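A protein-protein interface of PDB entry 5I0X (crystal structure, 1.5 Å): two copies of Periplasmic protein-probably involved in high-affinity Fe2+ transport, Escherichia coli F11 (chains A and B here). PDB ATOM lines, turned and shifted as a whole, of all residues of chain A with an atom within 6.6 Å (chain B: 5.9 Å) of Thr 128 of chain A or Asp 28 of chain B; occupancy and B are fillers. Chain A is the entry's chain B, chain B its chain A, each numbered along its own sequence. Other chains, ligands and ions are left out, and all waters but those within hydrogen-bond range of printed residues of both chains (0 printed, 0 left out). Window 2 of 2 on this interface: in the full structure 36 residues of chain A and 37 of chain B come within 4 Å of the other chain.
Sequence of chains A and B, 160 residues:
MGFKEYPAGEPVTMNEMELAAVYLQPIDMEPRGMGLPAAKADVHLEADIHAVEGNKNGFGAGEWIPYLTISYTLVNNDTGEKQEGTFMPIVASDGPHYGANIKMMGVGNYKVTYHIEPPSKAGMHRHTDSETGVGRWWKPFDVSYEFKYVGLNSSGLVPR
The side-chain hydroxyl of Thr 128 of chain A sits at hydrogen-bond distance from the backbone carbonyl oxygen of Asp 28 of chain B (2.8 Å).
The backbone NH (N) of Arg 126 of chain A is in hydrogen-bond range of the backbone carbonyl oxygen (O) of Glu 30 of chain B, 2.8 Å away.
The side-chain hydroxyl (OG1) of Thr 132 of chain A is in hydrogen-bond range of the side-chain carboxylate (OD1) of Asp 129 of chain A (2.6 Å).
The backbone carbonyl oxygen (O) of Ile 27 of chain B lies close to the side-chain amide oxygen (OD1) of Asn 101 of chain B.
OD1 of Asp 28 of chain B is in hydrogen-bond range of N of Ala 38 of chain B (3.2 Å).
The side-chain carboxylate (OD2) of Asp 129 of chain A is in hydrogen-bond range of the backbone NH (N) of Glu 131 of chain A, at 3.2 Å.
The backbone NH of Val 134 of chain A is in hydrogen-bond range of the backbone carbonyl oxygen of His 127 of chain A (3.0 Å).
The guanidinium group (NH2) of Arg 126 of chain A sits at hydrogen-bond distance from the backbone carbonyl oxygen (O) of Val 134 of chain A (2.9 Å).
Among the printed residues, merely in contact across the chains: Arg 126 of chain A with Met 29 of chain B (3.1 Å), His 127 of chain A with Ile 27 of chain B (3.5 Å), Asp 129 of chain A with Ile 27 of chain B (3.6 Å), Thr 128 of chain A with Glu 30 of chain B (3.6 Å), Thr 132 of chain A with Ile 27 of chain B (3.9 Å) and His 127 of chain A with Asp 28 of chain B (3.9 Å).
Printed residues of chain B within 4 Å of Thr 128 of chain A: Asp 28 (2.8 Å) and Glu 30 (3.6 Å).
Asp 28 of chain B touches just these residues of chain A: His 127 (3.9 Å) and Thr 128 (2.8 Å).
Of the printed residues of chain B, Asp 129 of chain A touches Ile 27 (3.6 Å).
Of the printed residues of chain A, Met 29 of chain B touches Arg 126 (3.1 Å).
Of the printed residues of chain B, Arg 126 of chain A touches Met 29 and Glu 30.
Of the printed residues of chain B, Thr 132 of chain A touches Ile 27 (3.9 Å).
Of the printed residues of chain B, His 127 of chain A touches Ile 27 (3.5 Å) and Asp 28 (3.9 Å).
Ala 38 of chain B touches none of the printed residues of chain A.
The nearest residue of chain A that does not touch Asp 28 of chain B is Arg 126 of chain A (4.1 Å).
Of the 9 printed residues of chain B, 4 touch a printed residue of chain A.
Among the printed residues, no Asp or Glu carboxylate lies within 4 Å of a Lys or Arg side-chain nitrogen of the other chain.
No position is printed for both chains.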
ATOM      1  N   ARG A 126      26.278 -27.475 -29.480  1.00  0.00           N
ATOM      2  CA  ARG A 126      26.606 -27.541 -28.061  1.00  0.00           C
ATOM      3  C   ARG A 126      25.394 -27.251 -27.177  1.00  0.00           C
ATOM      4  O   ARG A 126      24.604 -26.354 -27.487  1.00  0.00           O
ATOM      5  CB  ARG A 126      27.769 -26.588 -27.690  1.00  0.00           C
ATOM      6  CG  ARG A 126      27.562 -25.118 -28.002  1.00  0.00           C
ATOM      7  CD  ARG A 126      28.829 -24.313 -27.715  1.00  0.00           C
ATOM      8  NE  ARG A 126      28.621 -22.974 -28.252  1.00  0.00           N
ATOM      9  CZ  ARG A 126      28.117 -21.976 -27.533  1.00  0.00           C
ATOM     10  NH1 ARG A 126      27.921 -20.787 -28.087  1.00  0.00           N
ATOM     11  NH2 ARG A 126      27.844 -22.156 -26.254  1.00  0.00           N
ATOM     12  N   HIS A 127      25.270 -27.989 -26.080  1.00  0.00           N
ATOM     13  CA  HIS A 127      24.303 -27.628 -25.019  1.00  0.00           C
ATOM     14  C   HIS A 127      24.671 -26.282 -24.482  1.00  0.00           C
ATOM     15  O   HIS A 127      25.855 -25.971 -24.329  1.00  0.00           O
ATOM     16  CB  HIS A 127      24.333 -28.628 -23.864  1.00  0.00           C
ATOM     17  CG  HIS A 127      23.738 -29.986 -24.187  1.00  0.00           C
ATOM     18  ND1 HIS A 127      23.478 -30.903 -23.226  1.00  0.00           N
ATOM     19  CD2 HIS A 127      23.364 -30.557 -25.397  1.00  0.00           C
ATOM     20  CE1 HIS A 127      22.967 -32.022 -23.806  1.00  0.00           C
ATOM     21  NE2 HIS A 127      22.898 -31.805 -25.134  1.00  0.00           N
ATOM     22  N   THR A 128      23.657 -25.468 -24.192  1.00  0.00           N
ATOM     23  CA  THR A 128      23.877 -24.168 -23.524  1.00  0.00           C
ATOM     24  C   THR A 128      23.139 -24.019 -22.181  1.00  0.00           C
ATOM     25  O   THR A 128      23.173 -22.940 -21.593  1.00  0.00           O
ATOM     26  CB  THR A 128      23.564 -22.963 -24.449  1.00  0.00           C
ATOM     27  OG1 THR A 128      22.153 -22.864 -24.707  1.00  0.00           O
ATOM     28  CG2 THR A 128      24.318 -23.064 -25.769  1.00  0.00           C
ATOM     29  N   ASP A 129      22.483 -25.072 -21.692  1.00  0.00           N
ATOM     30  CA  ASP A 129      21.840 -25.031 -20.363  1.00  0.00           C
ATOM     31  C   ASP A 129      22.873 -24.890 -19.235  1.00  0.00           C
ATOM     32  O   ASP A 129      24.044 -25.193 -19.425  1.00  0.00           O
ATOM     33  CB  ASP A 129      20.991 -26.288 -20.140  1.00  0.00           C
ATOM     34  CG  ASP A 129      21.829 -27.545 -20.039  1.00  0.00           C
ATOM     35  OD1 ASP A 129      22.414 -27.949 -21.072  1.00  0.00           O
ATOM     36  OD2 ASP A 129      21.906 -28.131 -18.932  1.00  0.00           O
ATOM     37  N   SER A 130      22.451 -24.436 -18.053  1.00  0.00           N
ATOM     38  CA  SER A 130      23.407 -24.246 -16.957  1.00  0.00           C
ATOM     39  C   SER A 130      24.001 -25.551 -16.419  1.00  0.00           C
ATOM     40  O   SER A 130      25.163 -25.580 -16.005  1.00  0.00           O
ATOM     41  CB  SER A 130      22.804 -23.411 -15.817  1.00  0.00           C
ATOM     42  OG  SER A 130      21.700 -24.078 -15.231  1.00  0.00           O
ATOM     43  N   GLU A 131      23.219 -26.630 -16.455  1.00  0.00           N
ATOM     44  CA  GLU A 131      23.643 -27.918 -15.898  1.00  0.00           C
ATOM     45  C   GLU A 131      24.629 -28.707 -16.765  1.00  0.00           C
ATOM     46  O   GLU A 131      25.581 -29.289 -16.244  1.00  0.00           O
ATOM     47  CB  GLU A 131      22.433 -28.801 -15.574  1.00  0.00           C
ATOM     48  CG  GLU A 131      21.386 -28.146 -14.689  1.00  0.00           C
ATOM     49  CD  GLU A 131      20.208 -27.615 -15.482  1.00  0.00           C
ATOM     50  OE1 GLU A 131      19.069 -28.039 -15.195  1.00  0.00           O
ATOM     51  OE2 GLU A 131      20.418 -26.786 -16.394  1.00  0.00           O
ATOM     52  N   THR A 132      24.390 -28.748 -18.078  1.00  0.00           N
ATOM     53  CA  THR A 132      25.260 -29.514 -18.986  1.00  0.00           C
ATOM     54  C   THR A 132      25.902 -28.707 -20.113  1.00  0.00           C
ATOM     55  O   THR A 132      26.570 -29.271 -20.979  1.00  0.00           O
ATOM     56  CB  THR A 132      24.512 -30.715 -19.622  1.00  0.00           C
ATOM     57  OG1 THR A 132      23.521 -30.238 -20.533  1.00  0.00           O
ATOM     58  CG2 THR A 132      23.847 -31.588 -18.543  1.00  0.00           C
ATOM     59  N   GLY A 133      25.720 -27.396 -20.111  1.00  0.00           N
ATOM     60  CA  GLY A 133      26.181 -26.574 -21.221  1.00  0.00           C
ATOM     61  C   GLY A 133      27.688 -26.397 -21.246  1.00  0.00           C
ATOM     62  O   GLY A 133      28.364 -26.568 -20.229  1.00  0.00           O
ATOM     63  N   VAL A 134      28.196 -26.069 -22.426  1.00  0.00           N
ATOM     64  CA  VAL A 134      29.572 -25.571 -22.572  1.00  0.00           C
ATOM     65  C   VAL A 134      29.528 -24.241 -23.311  1.00  0.00           C
ATOM     66  O   VAL A 134      28.605 -23.958 -24.073  1.00  0.00           O
ATOM     67  CB  VAL A 134      30.512 -26.555 -23.305  1.00  0.00           C
ATOM     68  CG1 VAL A 134      30.806 -27.765 -22.436  1.00  0.00           C
ATOM     69  CG2 VAL A 134      29.918 -26.981 -24.631  1.00  0.00           C
ATOM     70  N   PRO B  26      13.998 -30.441 -22.899  1.00  0.00           N
ATOM     71  CA  PRO B  26      14.582 -29.793 -24.072  1.00  0.00           C
ATOM     72  C   PRO B  26      15.739 -28.857 -23.689  1.00  0.00           C
ATOM     73  O   PRO B  26      15.715 -28.240 -22.618  1.00  0.00           O
ATOM     74  CB  PRO B  26      13.410 -29.011 -24.683  1.00  0.00           C
ATOM     75  CG  PRO B  26      12.208 -29.746 -24.209  1.00  0.00           C
ATOM     76  CD  PRO B  26      12.537 -30.219 -22.834  1.00  0.00           C
ATOM     77  N   ILE B  27      16.758 -28.815 -24.539  1.00  0.00           N
ATOM     78  CA  ILE B  27      17.967 -28.037 -24.278  1.00  0.00           C
ATOM     79  C   ILE B  27      18.228 -27.066 -25.427  1.00  0.00           C
ATOM     80  O   ILE B  27      18.250 -27.454 -26.578  1.00  0.00           O
ATOM     81  CB  ILE B  27      19.169 -28.987 -24.054  1.00  0.00           C
ATOM     82  CG1 ILE B  27      18.976 -29.752 -22.745  1.00  0.00           C
ATOM     83  CG2 ILE B  27      20.489 -28.222 -24.069  1.00  0.00           C
ATOM     84  CD1 ILE B  27      20.119 -30.655 -22.357  1.00  0.00           C
ATOM     85  N   ASP B  28      18.420 -25.783 -25.125  1.00  0.00           N
ATOM     86  CA  ASP B  28      18.769 -24.856 -26.187  1.00  0.00           C
ATOM     87  C   ASP B  28      20.206 -25.092 -26.601  1.00  0.00           C
ATOM     88  O   ASP B  28      21.073 -25.278 -25.752  1.00  0.00           O
ATOM     89  CB  ASP B  28      18.518 -23.397 -25.790  1.00  0.00           C
ATOM     90  CG  ASP B  28      17.073 -22.983 -26.013  1.00  0.00           C
ATOM     91  OD1 ASP B  28      16.526 -23.236 -27.125  1.00  0.00           O
ATOM     92  OD2 ASP B  28      16.490 -22.404 -25.069  1.00  0.00           O
ATOM     93  N   MET B  29      20.433 -25.121 -27.904  1.00  0.00           N
ATOM     94  CA  MET B  29      21.752 -25.420 -28.438  1.00  0.00           C
ATOM     95  C   MET B  29      22.235 -24.321 -29.349  1.00  0.00           C
ATOM     96  O   MET B  29      21.427 -23.572 -29.910  1.00  0.00           O
ATOM     97  CB  MET B  29      21.739 -26.754 -29.191  1.00  0.00           C
ATOM     98  CG  MET B  29      21.550 -27.961 -28.279  1.00  0.00           C
ATOM     99  SD  MET B  29      21.647 -29.512 -29.209  1.00  0.00           S
ATOM    100  CE  MET B  29      20.005 -29.451 -29.925  1.00  0.00           C
ATOM    101  N   GLU B  30      23.556 -24.220 -29.474  1.00  0.00           N
ATOM    102  CA  GLU B  30      24.188 -23.348 -30.439  1.00  0.00           C
ATOM    103  C   GLU B  30      24.987 -24.203 -31.412  1.00  0.00           C
ATOM    104  O   GLU B  30      25.475 -25.258 -31.023  1.00  0.00           O
ATOM    105  CB  GLU B  30      25.116 -22.348 -29.742  1.00  0.00           C
ATOM    106  CG  GLU B  30      24.373 -21.301 -28.914  1.00  0.00           C
ATOM    107  CD  GLU B  30      23.726 -20.207 -29.747  1.00  0.00           C
ATOM    108  OE1 GLU B  30      22.905 -19.453 -29.176  1.00  0.00           O
ATOM    109  OE2 GLU B  30      24.026 -20.081 -30.954  1.00  0.00           O
ATOM    110  N   PRO B  37      13.936 -25.479 -31.742  1.00  0.00           N
ATOM    111  CA  PRO B  37      14.334 -24.801 -30.515  1.00  0.00           C
ATOM    112  C   PRO B  37      13.683 -25.455 -29.300  1.00  0.00           C
ATOM    113  O   PRO B  37      12.624 -26.105 -29.417  1.00  0.00           O
ATOM    114  CB  PRO B  37      13.809 -23.365 -30.692  1.00  0.00           C
ATOM    115  CG  PRO B  37      12.899 -23.394 -31.875  1.00  0.00           C
ATOM    116  CD  PRO B  37      13.271 -24.581 -32.704  1.00  0.00           C
ATOM    117  N   ALA B  38      14.317 -25.298 -28.143  1.00  0.00           N
ATOM    118  CA  ALA B  38      13.845 -25.952 -26.922  1.00  0.00           C
ATOM    119  C   ALA B  38      12.387 -25.638 -26.603  1.00  0.00           C
ATOM    120  O   ALA B  38      11.648 -26.518 -26.162  1.00  0.00           O
ATOM    121  CB  ALA B  38      14.740 -25.606 -25.742  1.00  0.00           C
ATOM    122  N   ALA B  39      11.983 -24.387 -26.844  1.00  0.00           N
ATOM    123  CA  ALA B  39      10.627 -23.928 -26.524  1.00  0.00           C
ATOM    124  C   ALA B  39       9.548 -24.659 -27.314  1.00  0.00           C
ATOM    125  O   ALA B  39       8.384 -24.689 -26.900  1.00  0.00           O
ATOM    126  CB  ALA B  39      10.510 -22.420 -26.740  1.00  0.00           C
ATOM    127  N   ASN B 101      16.445 -32.012 -30.097  1.00  0.00           N
ATOM    128  CA  ASN B 101      15.174 -31.698 -29.439  1.00  0.00           C
ATOM    129  C   ASN B 101      14.019 -32.272 -30.274  1.00  0.00           C
ATOM    130  O   ASN B 101      14.018 -32.160 -31.514  1.00  0.00           O
ATOM    131  CB  ASN B 101      15.007 -30.176 -29.285  1.00  0.00           C
ATOM    132  CG  ASN B 101      16.008 -29.555 -28.329  1.00  0.00           C
ATOM    133  OD1 ASN B 101      16.482 -28.427 -28.573  1.00  0.00           O
ATOM    134  ND2 ASN B 101      16.314 -30.237 -27.246  1.00  0.00           N
